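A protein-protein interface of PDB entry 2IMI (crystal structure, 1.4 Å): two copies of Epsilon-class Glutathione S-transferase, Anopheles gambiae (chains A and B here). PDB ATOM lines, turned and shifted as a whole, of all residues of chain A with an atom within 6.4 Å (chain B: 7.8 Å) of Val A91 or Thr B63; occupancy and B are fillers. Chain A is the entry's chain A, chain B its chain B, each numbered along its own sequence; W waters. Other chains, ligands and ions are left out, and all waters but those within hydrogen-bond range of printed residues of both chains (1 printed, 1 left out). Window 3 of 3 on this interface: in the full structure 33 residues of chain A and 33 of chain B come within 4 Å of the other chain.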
ATOM      1  N   LYS A  88      18.169  -3.622   7.800  1.00  0.00           N
ATOM      2  CA  LYS A  88      19.131  -2.808   8.524  1.00  0.00           C
ATOM      3  C   LYS A  88      18.852  -1.309   8.433  1.00  0.00           C
ATOM      4  O   LYS A  88      19.225  -0.557   9.333  1.00  0.00           O
ATOM      5  CB  LYS A  88      20.556  -3.152   8.082  1.00  0.00           C
ATOM      6  CG  LYS A  88      20.887  -4.591   8.438  1.00  0.00           C
ATOM      7  CD  LYS A  88      22.357  -4.856   8.622  1.00  0.00           C
ATOM      8  CE  LYS A  88      22.531  -6.227   9.256  1.00  0.00           C
ATOM      9  NZ  LYS A  88      23.956  -6.597   9.426  1.00  0.00           N
ATOM     10  N   ASP A  89      18.182  -0.880   7.368  1.00  0.00           N
ATOM     11  CA  ASP A  89      17.823   0.531   7.218  1.00  0.00           C
ATOM     12  C   ASP A  89      16.993   0.992   8.420  1.00  0.00           C
ATOM     13  O   ASP A  89      15.977   0.379   8.729  1.00  0.00           O
ATOM     14  CB  ASP A  89      17.014   0.735   5.941  1.00  0.00           C
ATOM     15  CG  ASP A  89      16.524   2.157   5.791  1.00  0.00           C
ATOM     16  OD1 ASP A  89      17.374   3.049   5.577  1.00  0.00           O
ATOM     17  OD2 ASP A  89      15.300   2.382   5.902  1.00  0.00           O
ATOM     18  N   PRO A  90      17.418   2.065   9.113  1.00  0.00           N
ATOM     19  CA  PRO A  90      16.684   2.474  10.327  1.00  0.00           C
ATOM     20  C   PRO A  90      15.186   2.711  10.154  1.00  0.00           C
ATOM     21  O   PRO A  90      14.409   2.317  11.035  1.00  0.00           O
ATOM     22  CB  PRO A  90      17.403   3.760  10.758  1.00  0.00           C
ATOM     23  CG  PRO A  90      18.797   3.600  10.211  1.00  0.00           C
ATOM     24  CD  PRO A  90      18.605   2.916   8.878  1.00  0.00           C
ATOM     25  N   VAL A  91      14.763   3.338   9.058  1.00  0.00           N
ATOM     26  CA  VAL A  91      13.339   3.646   8.878  1.00  0.00           C
ATOM     27  C   VAL A  91      12.523   2.389   8.540  1.00  0.00           C
ATOM     28  O   VAL A  91      11.489   2.130   9.165  1.00  0.00           O
ATOM     29  CB  VAL A  91      13.117   4.795   7.860  1.00  0.00           C
ATOM     30  CG1 VAL A  91      11.637   4.959   7.527  1.00  0.00           C
ATOM     31  CG2 VAL A  91      13.671   6.092   8.423  1.00  0.00           C
ATOM     32  N   LYS A  92      13.006   1.582   7.596  1.00  0.00           N
ATOM     33  CA  LYS A  92      12.337   0.315   7.299  1.00  0.00           C
ATOM     34  C   LYS A  92      12.316  -0.574   8.536  1.00  0.00           C
ATOM     35  O   LYS A  92      11.298  -1.209   8.828  1.00  0.00           O
ATOM     36  CB  LYS A  92      12.999  -0.421   6.135  1.00  0.00           C
ATOM     37  CG  LYS A  92      12.700   0.194   4.778  1.00  0.00           C
ATOM     38  CD  LYS A  92      13.555  -0.424   3.672  1.00  0.00           C
ATOM     39  CE  LYS A  92      13.224  -1.894   3.432  1.00  0.00           C
ATOM     40  NZ  LYS A  92      14.327  -2.613   2.715  1.00  0.00           N
ATOM     41  N   GLN A  93      13.426  -0.615   9.274  1.00  0.00           N
ATOM     42  CA  GLN A  93      13.477  -1.427  10.487  1.00  0.00           C
ATOM     43  C   GLN A  93      12.487  -0.942  11.526  1.00  0.00           C
ATOM     44  O   GLN A  93      11.892  -1.760  12.230  1.00  0.00           O
ATOM     45  CB  GLN A  93      14.869  -1.456  11.098  1.00  0.00           C
ATOM     46  CG  GLN A  93      15.039  -2.584  12.085  1.00  0.00           C
ATOM     47  CD  GLN A  93      16.324  -2.464  12.843  1.00  0.00           C
ATOM     48  OE1 GLN A  93      17.395  -2.860  12.358  1.00  0.00           O
ATOM     49  NE2 GLN A  93      16.245  -1.903  14.026  1.00  0.00           N
ATOM     50  N   ALA A  94      12.300   0.369  11.633  1.00  0.00           N
ATOM     51  CA  ALA A  94      11.353   0.903  12.614  1.00  0.00           C
ATOM     52  C   ALA A  94       9.942   0.413  12.372  1.00  0.00           C
ATOM     53  O   ALA A  94       9.221   0.128  13.324  1.00  0.00           O
ATOM     54  CB  ALA A  94      11.385   2.420  12.648  1.00  0.00           C
ATOM     55  N   ARG A  95       9.551   0.311  11.108  1.00  0.00           N
ATOM     56  CA  ARG A  95       8.225  -0.196  10.790  1.00  0.00           C
ATOM     57  C   ARG A  95       8.108  -1.672  11.181  1.00  0.00           C
ATOM     58  O   ARG A  95       7.076  -2.100  11.692  1.00  0.00           O
ATOM     59  CB  ARG A  95       7.891   0.024   9.314  1.00  0.00           C
ATOM     60  CG  ARG A  95       6.464  -0.312   8.958  1.00  0.00           C
ATOM     61  CD  ARG A  95       6.078   0.302   7.623  1.00  0.00           C
ATOM     62  NE  ARG A  95       4.752  -0.147   7.210  1.00  0.00           N
ATOM     63  CZ  ARG A  95       4.278  -0.052   5.971  1.00  0.00           C
ATOM     64  NH1 ARG A  95       3.062  -0.501   5.689  1.00  0.00           N
ATOM     65  NH2 ARG A  95       5.027   0.476   5.003  1.00  0.00           N
ATOM     66  N   VAL A  96       9.161  -2.455  10.962  1.00  0.00           N
ATOM     67  CA  VAL A  96       9.169  -3.864  11.398  1.00  0.00           C
ATOM     68  C   VAL A  96       9.137  -3.962  12.932  1.00  0.00           C
ATOM     69  O   VAL A  96       8.378  -4.756  13.486  1.00  0.00           O
ATOM     70  CB  VAL A  96      10.367  -4.654  10.804  1.00  0.00           C
ATOM     71  CG1 VAL A  96      10.332  -6.097  11.261  1.00  0.00           C
ATOM     72  CG2 VAL A  96      10.337  -4.595   9.278  1.00  0.00           C
ATOM     73  N   MET B   1      18.050  20.716  10.565  1.00  0.00           N
ATOM     74  CA  MET B   1      16.693  20.164  10.270  1.00  0.00           C
ATOM     75  C   MET B   1      15.743  20.393  11.460  1.00  0.00           C
ATOM     76  O   MET B   1      16.139  21.006  12.455  1.00  0.00           O
ATOM     77  CB  MET B   1      16.792  18.690   9.844  1.00  0.00           C
ATOM     78  CG  MET B   1      17.525  18.512   8.500  1.00  0.00           C
ATOM     79  SD  MET B   1      17.761  16.829   7.867  1.00  0.00           S
ATOM     80  CE  MET B   1      16.064  16.295   7.665  1.00  0.00           C
ATOM     81  N   LEU B   4      12.753  17.120  16.653  1.00  0.00           N
ATOM     82  CA  LEU B   4      11.881  15.955  16.732  1.00  0.00           C
ATOM     83  C   LEU B   4      10.561  16.339  17.384  1.00  0.00           C
ATOM     84  O   LEU B   4      10.536  17.115  18.341  1.00  0.00           O
ATOM     85  CB  LEU B   4      12.560  14.857  17.546  1.00  0.00           C
ATOM     86  CG  LEU B   4      13.892  14.335  17.002  1.00  0.00           C
ATOM     87  CD1 LEU B   4      14.705  13.691  18.102  1.00  0.00           C
ATOM     88  CD2 LEU B   4      13.669  13.360  15.863  1.00  0.00           C
ATOM     89  N   VAL B   5       9.474  15.802  16.844  1.00  0.00           N
ATOM     90  CA  VAL B   5       8.130  16.043  17.353  1.00  0.00           C
ATOM     91  C   VAL B   5       7.577  14.734  17.914  1.00  0.00           C
ATOM     92  O   VAL B   5       7.640  13.687  17.261  1.00  0.00           O
ATOM     93  CB  VAL B   5       7.204  16.573  16.241  1.00  0.00           C
ATOM     94  CG1 VAL B   5       5.756  16.641  16.711  1.00  0.00           C
ATOM     95  CG2 VAL B   5       7.695  17.949  15.740  1.00  0.00           C
ATOM     96  N   LEU B  49      -2.613   9.597  10.717  1.00  0.00           N
ATOM     97  CA  LEU B  49      -1.211   9.509  11.108  1.00  0.00           C
ATOM     98  C   LEU B  49      -0.815   8.144  11.708  1.00  0.00           C
ATOM     99  O   LEU B  49       0.260   7.623  11.427  1.00  0.00           O
ATOM    100  CB  LEU B  49      -0.891  10.644  12.090  1.00  0.00           C
ATOM    101  CG  LEU B  49       0.554  11.066  12.347  1.00  0.00           C
ATOM    102  CD1 LEU B  49       1.218  11.632  11.086  1.00  0.00           C
ATOM    103  CD2 LEU B  49       0.576  12.095  13.457  1.00  0.00           C
ATOM    104  N   VAL B  57       3.706   8.816  19.083  1.00  0.00           N
ATOM    105  CA  VAL B  57       4.064   8.820  17.671  1.00  0.00           C
ATOM    106  C   VAL B  57       5.146   9.878  17.485  1.00  0.00           C
ATOM    107  O   VAL B  57       5.011  11.009  17.971  1.00  0.00           O
ATOM    108  CB  VAL B  57       2.856   9.157  16.757  1.00  0.00           C
ATOM    109  CG1 VAL B  57       3.288   9.282  15.286  1.00  0.00           C
ATOM    110  CG2 VAL B  57       1.751   8.100  16.896  1.00  0.00           C
ATOM    111  N   LEU B  58       6.232   9.489  16.819  1.00  0.00           N
ATOM    112  CA  LEU B  58       7.322  10.403  16.491  1.00  0.00           C
ATOM    113  C   LEU B  58       7.194  10.893  15.060  1.00  0.00           C
ATOM    114  O   LEU B  58       6.902  10.118  14.160  1.00  0.00           O
ATOM    115  CB  LEU B  58       8.669   9.696  16.672  1.00  0.00           C
ATOM    116  CG  LEU B  58       9.938  10.517  16.413  1.00  0.00           C
ATOM    117  CD1 LEU B  58      10.255  11.427  17.601  1.00  0.00           C
ATOM    118  CD2 LEU B  58      11.099   9.598  16.111  1.00  0.00           C
ATOM    119  N   ASP B  59       7.393  12.196  14.880  1.00  0.00           N
ATOM    120  CA  ASP B  59       7.562  12.782  13.558  1.00  0.00           C
ATOM    121  C   ASP B  59       8.965  13.356  13.511  1.00  0.00           C
ATOM    122  O   ASP B  59       9.266  14.342  14.192  1.00  0.00           O
ATOM    123  CB  ASP B  59       6.507  13.867  13.292  1.00  0.00           C
ATOM    124  CG  ASP B  59       6.678  14.555  11.931  1.00  0.00           C
ATOM    125  OD1 ASP B  59       7.743  14.419  11.296  1.00  0.00           O
ATOM    126  OD2 ASP B  59       5.728  15.247  11.499  1.00  0.00           O
ATOM    127  N   ASP B  60       9.824  12.710  12.725  1.00  0.00           N
ATOM    128  CA  ASP B  60      11.184  13.184  12.488  1.00  0.00           C
ATOM    129  C   ASP B  60      11.286  13.685  11.059  1.00  0.00           C
ATOM    130  O   ASP B  60      11.523  12.912  10.129  1.00  0.00           O
ATOM    131  CB  ASP B  60      12.201  12.071  12.750  1.00  0.00           C
ATOM    132  CG  ASP B  60      13.637  12.523  12.550  1.00  0.00           C
ATOM    133  OD1 ASP B  60      14.546  11.682  12.697  1.00  0.00           O
ATOM    134  OD2 ASP B  60      13.882  13.715  12.246  1.00  0.00           O
ATOM    135  N   ASN B  61      11.086  14.992  10.894  1.00  0.00           N
ATOM    136  CA  ASN B  61      11.216  15.637   9.587  1.00  0.00           C
ATOM    137  C   ASN B  61      10.397  14.962   8.487  1.00  0.00           C
ATOM    138  O   ASN B  61      10.836  14.853   7.338  1.00  0.00           O
ATOM    139  CB  ASN B  61      12.694  15.780   9.213  1.00  0.00           C
ATOM    140  CG  ASN B  61      13.397  16.814  10.064  1.00  0.00           C
ATOM    141  OD1 ASN B  61      13.522  17.969   9.657  1.00  0.00           O
ATOM    142  ND2 ASN B  61      13.827  16.424  11.263  1.00  0.00           N
ATOM    143  N   GLY B  62       9.196  14.522   8.846  1.00  0.00           N
ATOM    144  CA  GLY B  62       8.293  13.878   7.900  1.00  0.00           C
ATOM    145  C   GLY B  62       8.235  12.366   8.027  1.00  0.00           C
ATOM    146  O   GLY B  62       7.272  11.742   7.571  1.00  0.00           O
ATOM    147  N   THR B  63       9.268  11.784   8.639  1.00  0.00           N
ATOM    148  CA  THR B  63       9.312  10.350   8.917  1.00  0.00           C
ATOM    149  C   THR B  63       8.474  10.056  10.162  1.00  0.00           C
ATOM    150  O   THR B  63       8.771  10.550  11.253  1.00  0.00           O
ATOM    151  CB  THR B  63      10.756   9.869   9.147  1.00  0.00           C
ATOM    152  OG1 THR B  63      11.526  10.085   7.957  1.00  0.00           O
ATOM    153  CG2 THR B  63      10.799   8.385   9.510  1.00  0.00           C
ATOM    154  N   ILE B  64       7.427   9.256   9.979  1.00  0.00           N
ATOM    155  CA  ILE B  64       6.499   8.924  11.060  1.00  0.00           C
ATOM    156  C   ILE B  64       6.801   7.547  11.624  1.00  0.00           C
ATOM    157  O   ILE B  64       6.798   6.556  10.895  1.00  0.00           O
ATOM    158  CB  ILE B  64       5.016   8.984  10.587  1.00  0.00           C
ATOM    159  CG1 ILE B  64       4.689  10.337   9.931  1.00  0.00           C
ATOM    160  CG2 ILE B  64       4.051   8.690  11.749  1.00  0.00           C
ATOM    161  CD1 ILE B  64       5.018  11.556  10.784  1.00  0.00           C
ATOM    162  N   ILE B  65       7.060   7.487  12.927  1.00  0.00           N
ATOM    163  CA  ILE B  65       7.275   6.202  13.588  1.00  0.00           C
ATOM    164  C   ILE B  65       6.303   6.062  14.728  1.00  0.00           C
ATOM    165  O   ILE B  65       6.173   6.945  15.578  1.00  0.00           O
ATOM    166  CB  ILE B  65       8.715   6.029  14.087  1.00  0.00           C
ATOM    167  CG1 ILE B  65       9.675   6.119  12.911  1.00  0.00           C
ATOM    168  CG2 ILE B  65       8.885   4.673  14.804  1.00  0.00           C
ATOM    169  CD1 ILE B  65      11.089   6.238  13.316  1.00  0.00           C
ATOM    170  N   THR B  66       5.585   4.958  14.703  1.00  0.00           N
ATOM    171  CA  THR B  66       4.711   4.625  15.768  1.00  0.00           C
ATOM    172  C   THR B  66       5.461   3.645  16.663  1.00  0.00           C
ATOM    173  O   THR B  66       6.483   3.049  16.283  1.00  0.00           O
ATOM    174  CB  THR B  66       3.426   3.989  15.232  1.00  0.00           C
ATOM    175  OG1 THR B  66       3.758   2.806  14.490  1.00  0.00           O
ATOM    176  CG2 THR B  66       2.708   4.972  14.314  1.00  0.00           C
ATOM    177  N   TYR B  74      15.007   3.648  17.110  1.00  0.00           N
ATOM    178  CA  TYR B  74      15.327   4.619  16.062  1.00  0.00           C
ATOM    179  C   TYR B  74      16.153   5.793  16.593  1.00  0.00           C
ATOM    180  O   TYR B  74      17.134   6.203  15.956  1.00  0.00           O
ATOM    181  CB  TYR B  74      14.031   5.109  15.429  1.00  0.00           C
ATOM    182  CG  TYR B  74      14.175   6.206  14.408  1.00  0.00           C
ATOM    183  CD1 TYR B  74      14.453   5.920  13.071  1.00  0.00           C
ATOM    184  CD2 TYR B  74      13.996   7.536  14.778  1.00  0.00           C
ATOM    185  CE1 TYR B  74      14.558   6.937  12.127  1.00  0.00           C
ATOM    186  CE2 TYR B  74      14.089   8.554  13.846  1.00  0.00           C
ATOM    187  CZ  TYR B  74      14.377   8.247  12.528  1.00  0.00           C
ATOM    188  OH  TYR B  74      14.476   9.259  11.597  1.00  0.00           O
ATOM    189  N   THR B  77      19.653   4.632  17.447  1.00  0.00           N
ATOM    190  CA  THR B  77      20.327   4.271  16.190  1.00  0.00           C
ATOM    191  C   THR B  77      20.808   5.499  15.425  1.00  0.00           C
ATOM    192  O   THR B  77      21.960   5.541  14.973  1.00  0.00           O
ATOM    193  CB  THR B  77      19.411   3.434  15.255  1.00  0.00           C
ATOM    194  OG1 THR B  77      19.036   2.210  15.900  1.00  0.00           O
ATOM    195  CG2 THR B  77      20.116   3.095  13.932  1.00  0.00           C
ATOM    196  N   LYS B  78      19.932   6.485  15.278  1.00  0.00           N
ATOM    197  CA  LYS B  78      20.208   7.644  14.432  1.00  0.00           C
ATOM    198  C   LYS B  78      20.939   8.755  15.165  1.00  0.00           C
ATOM    199  O   LYS B  78      21.801   9.422  14.571  1.00  0.00           O
ATOM    200  CB  LYS B  78      18.908   8.193  13.832  1.00  0.00           C
ATOM    201  CG  LYS B  78      19.121   9.242  12.745  1.00  0.00           C
ATOM    202  CD  LYS B  78      17.830   9.542  11.991  1.00  0.00           C
ATOM    203  CE  LYS B  78      18.029  10.665  10.972  1.00  0.00           C
ATOM    204  NZ  LYS B  78      18.877  10.249   9.822  1.00  0.00           N
ATOM    205  N   TYR B  79      20.615   8.950  16.440  1.00  0.00           N
ATOM    206  CA  TYR B  79      21.059  10.149  17.165  1.00  0.00           C
ATOM    207  C   TYR B  79      21.961   9.899  18.370  1.00  0.00           C
ATOM    208  O   TYR B  79      22.486  10.850  18.952  1.00  0.00           O
ATOM    209  CB  TYR B  79      19.851  11.001  17.570  1.00  0.00           C
ATOM    210  CG  TYR B  79      19.036  11.461  16.385  1.00  0.00           C
ATOM    211  CD1 TYR B  79      19.562  12.374  15.467  1.00  0.00           C
ATOM    212  CD2 TYR B  79      17.747  10.971  16.164  1.00  0.00           C
ATOM    213  CE1 TYR B  79      18.831  12.789  14.372  1.00  0.00           C
ATOM    214  CE2 TYR B  79      16.999  11.388  15.066  1.00  0.00           C
ATOM    215  CZ  TYR B  79      17.548  12.298  14.176  1.00  0.00           C
ATOM    216  OH  TYR B  79      16.824  12.716  13.085  1.00  0.00           O
HETATM  217  O   HOH W   1      17.500   0.612  13.908  1.00  0.00           O
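Asp A89 touches none of the printed residues of chain B.
Of the printed residues of chain B, Pro A90 touches Thr B77 (3.98 Å).
Val A91 touches two residues of chain B.
Of the printed residues of chain B, Ala A94 touches Ile B65 (3.9 Å).
Of the printed residues of chain A, Tyr B74 touches Val A91 (3.9 Å).
The nearest residue of chain B that does not touch Val A91 is Ile B65 (5.5 Å).
Water W1 lies within hydrogen-bond range of NE2 of Gln A93 (2.8 Å) and OG1 of Thr B77 (3.0 Å).
No position is printed for both chains.
Among the printed residues, merely in contact across the chains: Pro A90 with Thr B77 (3.98 Å), Val A91 with Thr B63 (3.8 Å), Val A91 with Tyr B74 (3.9 Å) and Ala A94 with Ile B65 (3.9 Å).
The backbone NH of Val A91 lies close to the side-chain carboxylate of Asp A89 (3.3 Å).
N of Leu B58 is in hydrogen-bond range of O of Ile B65, at 2.8 Å.
The side-chain carboxylate of Asp B60 lies within hydrogen-bond range of the side-chain hydroxyl of Tyr B74.
Of the 9 printed residues of chain A, 3 touch a printed residue of chain B.
Hydrophobic or aromatic side chains of chain A within 4 Å of the printed part of chain B: Pro A90, Val A91 and Ala A94.
Of the 18 printed residues of chain B, 4 touch a printed residue of chain A.
Hydrophobic or aromatic side chains of chain B that line the printed part of chain A: Ile B65 and Tyr B74.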
